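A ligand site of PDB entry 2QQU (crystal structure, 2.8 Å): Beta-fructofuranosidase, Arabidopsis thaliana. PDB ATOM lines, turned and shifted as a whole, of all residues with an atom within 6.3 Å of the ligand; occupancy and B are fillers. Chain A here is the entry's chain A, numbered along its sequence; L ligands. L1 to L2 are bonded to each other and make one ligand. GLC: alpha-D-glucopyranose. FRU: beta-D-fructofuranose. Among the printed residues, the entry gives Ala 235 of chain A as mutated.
NH1 of Arg 144 lies close to O3 of FRU L2 (3.1 Å). O6 of FRU L2 is in hydrogen-bond range of OE1 of Gln 35 (2.7 Å). NE1 of Trp 43 is in hydrogen-bond range of O6 of FRU L2 (3.0 Å). An oxygen (O4) of FRU L2 sits close to the side-chain hydroxyl (OG) of Ser 79 (3.5 Å). The side-chain carboxylate (OD1) of Asp 145 is in hydrogen-bond range of an oxygen (O4) of FRU L2. The backbone NH (N) of Ser 79 sits at hydrogen-bond distance from an oxygen (O4) of FRU L2 (3.2 Å). The side-chain amide nitrogen of Asn 18 sits at hydrogen-bond distance from an oxygen (O6) of FRU L2, at 2.8 Å. O1 of FRU L2 is in hydrogen-bond range of OD1 of Asp 19 (2.5 Å). OE2 of Glu 199 sits at hydrogen-bond distance from O2 of GLC L1 (2.7 Å).
The backbone NH of Asp 145 sits at hydrogen-bond distance from the side-chain hydroxyl of Thr 95 (2.7 Å). The backbone NH of Gln 35 is in hydrogen-bond range of the backbone carbonyl oxygen of Asp 19, at 3.0 Å. The side-chain amide nitrogen of Gln 35 is in hydrogen-bond range of the backbone carbonyl oxygen of Cys 77, at 3.0 Å. OD2 of Asp 19 is in hydrogen-bond range of OG of Ser 79 (3.0 Å). The side-chain amide nitrogen of Asn 18 lies close to the indole nitrogen of Trp 43 (3.3 Å). OH of Tyr 275 lies within hydrogen-bond range of OE1 of Glu 199. The side-chain carboxylate (OD2) of Asp 145 is in hydrogen-bond range of the backbone NH (N) of Cys 200 (2.7 Å). NH2 of Arg 144 is in hydrogen-bond range of O of Ser 141 (3.4 Å).
Trp 78 touches the ligand. NZ of Lys 238 touches O2 of GLC L1, at 3.9 Å. CZ3 of Trp 293 touches O1 of FRU L2, at 3.7 Å. Hydrophobic or aromatic side chains within 4 Å of the ligand: Trp 43, Trp 78 and Trp 293. Of the 22 residues printed, 11 come within 4 Å of the ligand. Along chain A the residues within 4 Å of the ligand span positions 18 to 293.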
ATOM      1  N   ASN A  18      19.172   4.263  26.327  1.00  0.00           N
ATOM      2  CA  ASN A  18      20.420   4.362  25.623  1.00  0.00           C
ATOM      3  C   ASN A  18      20.056   4.757  24.179  1.00  0.00           C
ATOM      4  O   ASN A  18      19.025   5.415  23.987  1.00  0.00           O
ATOM      5  CB  ASN A  18      21.068   2.965  25.733  1.00  0.00           C
ATOM      6  CG  ASN A  18      22.423   2.873  25.109  1.00  0.00           C
ATOM      7  OD1 ASN A  18      23.118   3.871  24.921  1.00  0.00           O
ATOM      8  ND2 ASN A  18      22.831   1.652  24.777  1.00  0.00           N
ATOM      9  N   ASP A  19      20.850   4.383  23.181  1.00  0.00           N
ATOM     10  CA  ASP A  19      20.647   4.766  21.777  1.00  0.00           C
ATOM     11  C   ASP A  19      19.191   4.720  21.290  1.00  0.00           C
ATOM     12  O   ASP A  19      18.450   3.799  21.638  1.00  0.00           O
ATOM     13  CB  ASP A  19      21.469   3.860  20.864  1.00  0.00           C
ATOM     14  CG  ASP A  19      22.963   4.084  20.996  1.00  0.00           C
ATOM     15  OD1 ASP A  19      23.440   4.465  22.088  1.00  0.00           O
ATOM     16  OD2 ASP A  19      23.673   3.850  19.993  1.00  0.00           O
ATOM     17  N   GLN A  35      17.610   1.081  22.729  1.00  0.00           N
ATOM     18  CA  GLN A  35      18.400   0.203  23.586  1.00  0.00           C
ATOM     19  C   GLN A  35      17.866   0.283  24.998  1.00  0.00           C
ATOM     20  O   GLN A  35      17.882   1.354  25.614  1.00  0.00           O
ATOM     21  CB  GLN A  35      19.876   0.585  23.536  1.00  0.00           C
ATOM     22  CG  GLN A  35      20.504   0.533  22.145  1.00  0.00           C
ATOM     23  CD  GLN A  35      20.816  -0.883  21.702  1.00  0.00           C
ATOM     24  OE1 GLN A  35      21.787  -1.479  22.169  1.00  0.00           O
ATOM     25  NE2 GLN A  35      20.025  -1.408  20.780  1.00  0.00           N
ATOM     26  N   TRP A  43      23.793   0.012  31.857  1.00  0.00           N
ATOM     27  CA  TRP A  43      23.866  -0.741  30.590  1.00  0.00           C
ATOM     28  C   TRP A  43      23.927  -2.255  30.830  1.00  0.00           C
ATOM     29  O   TRP A  43      24.605  -2.722  31.751  1.00  0.00           O
ATOM     30  CB  TRP A  43      25.064  -0.290  29.741  1.00  0.00           C
ATOM     31  CG  TRP A  43      24.991  -0.776  28.314  1.00  0.00           C
ATOM     32  CD1 TRP A  43      24.426  -0.119  27.260  1.00  0.00           C
ATOM     33  CD2 TRP A  43      25.451  -2.035  27.800  1.00  0.00           C
ATOM     34  NE1 TRP A  43      24.519  -0.885  26.120  1.00  0.00           N
ATOM     35  CE2 TRP A  43      25.138  -2.058  26.415  1.00  0.00           C
ATOM     36  CE3 TRP A  43      26.112  -3.153  28.363  1.00  0.00           C
ATOM     37  CZ2 TRP A  43      25.452  -3.155  25.586  1.00  0.00           C
ATOM     38  CZ3 TRP A  43      26.422  -4.227  27.540  1.00  0.00           C
ATOM     39  CH2 TRP A  43      26.108  -4.224  26.173  1.00  0.00           C
ATOM     40  N   ILE A  46      20.906  -5.964  26.705  1.00  0.00           N
ATOM     41  CA  ILE A  46      20.338  -4.914  25.876  1.00  0.00           C
ATOM     42  C   ILE A  46      19.422  -5.421  24.767  1.00  0.00           C
ATOM     43  O   ILE A  46      19.793  -6.330  24.008  1.00  0.00           O
ATOM     44  CB  ILE A  46      21.440  -3.942  25.388  1.00  0.00           C
ATOM     45  CG1 ILE A  46      20.892  -2.507  25.318  1.00  0.00           C
ATOM     46  CG2 ILE A  46      22.124  -4.414  24.090  1.00  0.00           C
ATOM     47  CD1 ILE A  46      20.791  -1.821  26.686  1.00  0.00           C
ATOM     48  N   CYS A  77      21.473  -7.328  21.367  1.00  0.00           N
ATOM     49  CA  CYS A  77      20.894  -6.649  20.205  1.00  0.00           C
ATOM     50  C   CYS A  77      21.221  -5.150  20.227  1.00  0.00           C
ATOM     51  O   CYS A  77      20.483  -4.329  20.798  1.00  0.00           O
ATOM     52  CB  CYS A  77      19.383  -6.866  20.141  1.00  0.00           C
ATOM     53  SG  CYS A  77      18.933  -8.586  19.901  1.00  0.00           S
ATOM     54  N   TRP A  78      22.340  -4.809  19.596  1.00  0.00           N
ATOM     55  CA  TRP A  78      22.840  -3.444  19.589  1.00  0.00           C
ATOM     56  C   TRP A  78      22.090  -2.577  18.572  1.00  0.00           C
ATOM     57  O   TRP A  78      21.028  -2.951  18.083  1.00  0.00           O
ATOM     58  CB  TRP A  78      24.361  -3.429  19.398  1.00  0.00           C
ATOM     59  CG  TRP A  78      25.112  -4.004  20.563  1.00  0.00           C
ATOM     60  CD1 TRP A  78      24.603  -4.790  21.553  1.00  0.00           C
ATOM     61  CD2 TRP A  78      26.514  -3.853  20.854  1.00  0.00           C
ATOM     62  NE1 TRP A  78      25.585  -5.139  22.447  1.00  0.00           N
ATOM     63  CE2 TRP A  78      26.763  -4.586  22.041  1.00  0.00           C
ATOM     64  CE3 TRP A  78      27.572  -3.193  20.228  1.00  0.00           C
ATOM     65  CZ2 TRP A  78      28.041  -4.658  22.616  1.00  0.00           C
ATOM     66  CZ3 TRP A  78      28.831  -3.260  20.807  1.00  0.00           C
ATOM     67  CH2 TRP A  78      29.057  -3.990  21.984  1.00  0.00           C
ATOM     68  N   SER A  79      22.639  -1.405  18.280  1.00  0.00           N
ATOM     69  CA  SER A  79      21.910  -0.410  17.498  1.00  0.00           C
ATOM     70  C   SER A  79      21.779  -0.740  16.015  1.00  0.00           C
ATOM     71  O   SER A  79      22.483  -1.606  15.485  1.00  0.00           O
ATOM     72  CB  SER A  79      22.540   0.959  17.682  1.00  0.00           C
ATOM     73  OG  SER A  79      22.392   1.372  19.019  1.00  0.00           O
ATOM     74  N   GLY A  80      20.852  -0.035  15.366  1.00  0.00           N
ATOM     75  CA  GLY A  80      20.573  -0.213  13.962  1.00  0.00           C
ATOM     76  C   GLY A  80      19.462   0.700  13.474  1.00  0.00           C
ATOM     77  O   GLY A  80      18.976   1.565  14.227  1.00  0.00           O
ATOM     78  N   THR A  95      22.866  -4.504  14.666  1.00  0.00           N
ATOM     79  CA  THR A  95      24.087  -5.182  15.067  1.00  0.00           C
ATOM     80  C   THR A  95      23.767  -6.193  16.173  1.00  0.00           C
ATOM     81  O   THR A  95      23.161  -5.839  17.192  1.00  0.00           O
ATOM     82  CB  THR A  95      25.135  -4.173  15.589  1.00  0.00           C
ATOM     83  OG1 THR A  95      25.527  -3.287  14.526  1.00  0.00           O
ATOM     84  CG2 THR A  95      26.371  -4.892  16.123  1.00  0.00           C
ATOM     85  N   GLN A 103      30.712  -8.479  16.540  1.00  0.00           N
ATOM     86  CA  GLN A 103      29.683  -7.561  16.093  1.00  0.00           C
ATOM     87  C   GLN A 103      29.348  -7.846  14.633  1.00  0.00           C
ATOM     88  O   GLN A 103      30.205  -7.718  13.754  1.00  0.00           O
ATOM     89  CB  GLN A 103      30.133  -6.119  16.284  1.00  0.00           C
ATOM     90  CG  GLN A 103      29.980  -5.610  17.706  1.00  0.00           C
ATOM     91  CD  GLN A 103      31.010  -4.550  18.066  1.00  0.00           C
ATOM     92  OE1 GLN A 103      31.499  -3.813  17.202  1.00  0.00           O
ATOM     93  NE2 GLN A 103      31.329  -4.470  19.356  1.00  0.00           N
ATOM     94  N   SER A 141      35.357  -6.422  16.948  1.00  0.00           N
ATOM     95  CA  SER A 141      34.979  -5.807  18.201  1.00  0.00           C
ATOM     96  C   SER A 141      34.583  -4.342  17.965  1.00  0.00           C
ATOM     97  O   SER A 141      34.188  -3.635  18.898  1.00  0.00           O
ATOM     98  CB  SER A 141      36.131  -5.905  19.198  1.00  0.00           C
ATOM     99  OG  SER A 141      35.666  -5.665  20.505  1.00  0.00           O
ATOM    100  N   ARG A 144      29.814  -1.905  14.170  1.00  0.00           N
ATOM    101  CA  ARG A 144      28.417  -1.785  14.589  1.00  0.00           C
ATOM    102  C   ARG A 144      27.638  -0.607  13.986  1.00  0.00           C
ATOM    103  O   ARG A 144      28.218   0.327  13.423  1.00  0.00           O
ATOM    104  CB  ARG A 144      28.324  -1.790  16.121  1.00  0.00           C
ATOM    105  CG  ARG A 144      28.789  -0.537  16.797  1.00  0.00           C
ATOM    106  CD  ARG A 144      29.124  -0.818  18.227  1.00  0.00           C
ATOM    107  NE  ARG A 144      30.544  -1.072  18.385  1.00  0.00           N
ATOM    108  CZ  ARG A 144      31.350  -0.361  19.160  1.00  0.00           C
ATOM    109  NH1 ARG A 144      30.870   0.638  19.889  1.00  0.00           N
ATOM    110  NH2 ARG A 144      32.635  -0.669  19.215  1.00  0.00           N
ATOM    111  N   ASP A 145      26.310  -0.691  14.123  1.00  0.00           N
ATOM    112  CA  ASP A 145      25.362   0.384  13.808  1.00  0.00           C
ATOM    113  C   ASP A 145      25.187   0.645  12.310  1.00  0.00           C
ATOM    114  O   ASP A 145      25.633   1.680  11.800  1.00  0.00           O
ATOM    115  CB  ASP A 145      25.720   1.686  14.522  1.00  0.00           C
ATOM    116  CG  ASP A 145      26.085   1.468  15.975  1.00  0.00           C
ATOM    117  OD1 ASP A 145      25.686   0.423  16.527  1.00  0.00           O
ATOM    118  OD2 ASP A 145      26.749   2.346  16.564  1.00  0.00           O
ATOM    119  N   MET A 197      36.850   5.034  17.051  1.00  0.00           N
ATOM    120  CA  MET A 197      35.668   4.338  16.543  1.00  0.00           C
ATOM    121  C   MET A 197      34.596   5.331  16.052  1.00  0.00           C
ATOM    122  O   MET A 197      34.401   6.392  16.663  1.00  0.00           O
ATOM    123  CB  MET A 197      35.111   3.433  17.643  1.00  0.00           C
ATOM    124  CG  MET A 197      33.784   2.743  17.355  1.00  0.00           C
ATOM    125  SD  MET A 197      33.833   1.754  15.857  1.00  0.00           S
ATOM    126  CE  MET A 197      32.170   1.121  15.829  1.00  0.00           C
ATOM    127  N   GLU A 199      30.797   5.502  15.816  1.00  0.00           N
ATOM    128  CA  GLU A 199      29.552   4.864  16.246  1.00  0.00           C
ATOM    129  C   GLU A 199      28.365   5.506  15.514  1.00  0.00           C
ATOM    130  O   GLU A 199      28.536   6.525  14.831  1.00  0.00           O
ATOM    131  CB  GLU A 199      29.386   4.960  17.767  1.00  0.00           C
ATOM    132  CG  GLU A 199      30.405   4.172  18.566  1.00  0.00           C
ATOM    133  CD  GLU A 199      30.132   4.178  20.070  1.00  0.00           C
ATOM    134  OE1 GLU A 199      29.676   5.213  20.601  1.00  0.00           O
ATOM    135  OE2 GLU A 199      30.365   3.130  20.715  1.00  0.00           O
ATOM    136  N   CYS A 200      27.180   4.905  15.657  1.00  0.00           N
ATOM    137  CA  CYS A 200      25.940   5.395  15.049  1.00  0.00           C
ATOM    138  C   CYS A 200      26.125   6.378  13.872  1.00  0.00           C
ATOM    139  O   CYS A 200      25.782   7.559  13.985  1.00  0.00           O
ATOM    140  CB  CYS A 200      25.010   6.014  16.134  1.00  0.00           C
ATOM    141  SG  CYS A 200      23.516   5.030  16.605  1.00  0.00           S
ATOM    142  N   ALA A 235      33.319   8.078  19.382  1.00  0.00           N
ATOM    143  CA  ALA A 235      33.422   7.334  20.638  1.00  0.00           C
ATOM    144  C   ALA A 235      34.363   7.976  21.660  1.00  0.00           C
ATOM    145  O   ALA A 235      34.041   8.073  22.844  1.00  0.00           O
ATOM    146  CB  ALA A 235      33.834   5.896  20.366  1.00  0.00           C
ATOM    147  N   LYS A 238      32.912  11.431  22.714  1.00  0.00           N
ATOM    148  CA  LYS A 238      31.515  11.274  23.136  1.00  0.00           C
ATOM    149  C   LYS A 238      30.612  12.415  22.643  1.00  0.00           C
ATOM    150  O   LYS A 238      29.762  12.921  23.390  1.00  0.00           O
ATOM    151  CB  LYS A 238      31.384  11.071  24.655  1.00  0.00           C
ATOM    152  CG  LYS A 238      32.051   9.792  25.170  1.00  0.00           C
ATOM    153  CD  LYS A 238      31.052   8.664  25.400  1.00  0.00           C
ATOM    154  CE  LYS A 238      31.762   7.312  25.506  1.00  0.00           C
ATOM    155  NZ  LYS A 238      31.892   6.689  24.161  1.00  0.00           N
ATOM    156  N   TYR A 275      23.950  12.364  22.251  1.00  0.00           N
ATOM    157  CA  TYR A 275      24.703  11.272  21.649  1.00  0.00           C
ATOM    158  C   TYR A 275      23.862  10.276  20.871  1.00  0.00           C
ATOM    159  O   TYR A 275      22.639  10.226  21.033  1.00  0.00           O
ATOM    160  CB  TYR A 275      25.539  10.562  22.710  1.00  0.00           C
ATOM    161  CG  TYR A 275      26.714   9.828  22.139  1.00  0.00           C
ATOM    162  CD1 TYR A 275      27.795  10.525  21.591  1.00  0.00           C
ATOM    163  CD2 TYR A 275      26.756   8.438  22.121  1.00  0.00           C
ATOM    164  CE1 TYR A 275      28.873   9.844  21.049  1.00  0.00           C
ATOM    165  CE2 TYR A 275      27.834   7.751  21.587  1.00  0.00           C
ATOM    166  CZ  TYR A 275      28.889   8.462  21.051  1.00  0.00           C
ATOM    167  OH  TYR A 275      29.957   7.778  20.518  1.00  0.00           O
ATOM    168  N   ALA A 276      24.527   9.498  20.020  1.00  0.00           N
ATOM    169  CA  ALA A 276      23.915   8.468  19.176  1.00  0.00           C
ATOM    170  C   ALA A 276      22.736   8.934  18.309  1.00  0.00           C
ATOM    171  O   ALA A 276      21.773   8.195  18.131  1.00  0.00           O
ATOM    172  CB  ALA A 276      23.523   7.269  20.013  1.00  0.00           C
ATOM    173  N   TRP A 293      20.033  10.900  22.000  1.00  0.00           N
ATOM    174  CA  TRP A 293      20.085  10.325  23.334  1.00  0.00           C
ATOM    175  C   TRP A 293      20.873  11.220  24.288  1.00  0.00           C
ATOM    176  O   TRP A 293      22.085  11.404  24.128  1.00  0.00           O
ATOM    177  CB  TRP A 293      20.657   8.904  23.289  1.00  0.00           C
ATOM    178  CG  TRP A 293      21.132   8.372  24.602  1.00  0.00           C
ATOM    179  CD1 TRP A 293      20.443   8.367  25.787  1.00  0.00           C
ATOM    180  CD2 TRP A 293      22.389   7.731  24.868  1.00  0.00           C
ATOM    181  NE1 TRP A 293      21.199   7.785  26.770  1.00  0.00           N
ATOM    182  CE2 TRP A 293      22.395   7.382  26.237  1.00  0.00           C
ATOM    183  CE3 TRP A 293      23.509   7.427  24.084  1.00  0.00           C
ATOM    184  CZ2 TRP A 293      23.485   6.746  26.836  1.00  0.00           C
ATOM    185  CZ3 TRP A 293      24.590   6.793  24.685  1.00  0.00           C
ATOM    186  CH2 TRP A 293      24.576   6.461  26.042  1.00  0.00           C
HETATM  187  C1  GLC L   1      27.959   1.870  23.423  1.00  0.00           C
HETATM  188  C2  GLC L   1      29.348   2.357  23.846  1.00  0.00           C
HETATM  189  C3  GLC L   1      30.412   1.341  23.424  1.00  0.00           C
HETATM  190  C4  GLC L   1      30.083  -0.059  23.944  1.00  0.00           C
HETATM  191  C5  GLC L   1      28.615  -0.432  23.686  1.00  0.00           C
HETATM  192  C6  GLC L   1      28.241  -1.668  24.494  1.00  0.00           C
HETATM  193  O2  GLC L   1      29.616   3.622  23.274  1.00  0.00           O
HETATM  194  O3  GLC L   1      31.697   1.721  23.866  1.00  0.00           O
HETATM  195  O4  GLC L   1      30.915  -1.011  23.310  1.00  0.00           O
HETATM  196  O5  GLC L   1      27.706   0.606  24.021  1.00  0.00           O
HETATM  197  O6  GLC L   1      28.968  -1.736  25.694  1.00  0.00           O
HETATM  198  C1  FRU L   2      26.724   3.803  21.275  1.00  0.00           C
HETATM  199  C2  FRU L   2      26.719   2.275  21.341  1.00  0.00           C
HETATM  200  C3  FRU L   2      26.680   1.697  19.932  1.00  0.00           C
HETATM  201  C4  FRU L   2      26.097   0.333  20.166  1.00  0.00           C
HETATM  202  C5  FRU L   2      25.116   0.598  21.296  1.00  0.00           C
HETATM  203  C6  FRU L   2      25.090  -0.547  22.297  1.00  0.00           C
HETATM  204  O1  FRU L   2      25.904   4.298  22.315  1.00  0.00           O
HETATM  205  O2  FRU L   2      27.885   1.792  21.993  1.00  0.00           O
HETATM  206  O3  FRU L   2      27.961   1.582  19.391  1.00  0.00           O
HETATM  207  O4  FRU L   2      25.493  -0.186  19.008  1.00  0.00           O
HETATM  208  O5  FRU L   2      25.539   1.775  21.952  1.00  0.00           O
HETATM  209  O6  FRU L   2      24.037  -0.306  23.182  1.00  0.00           O
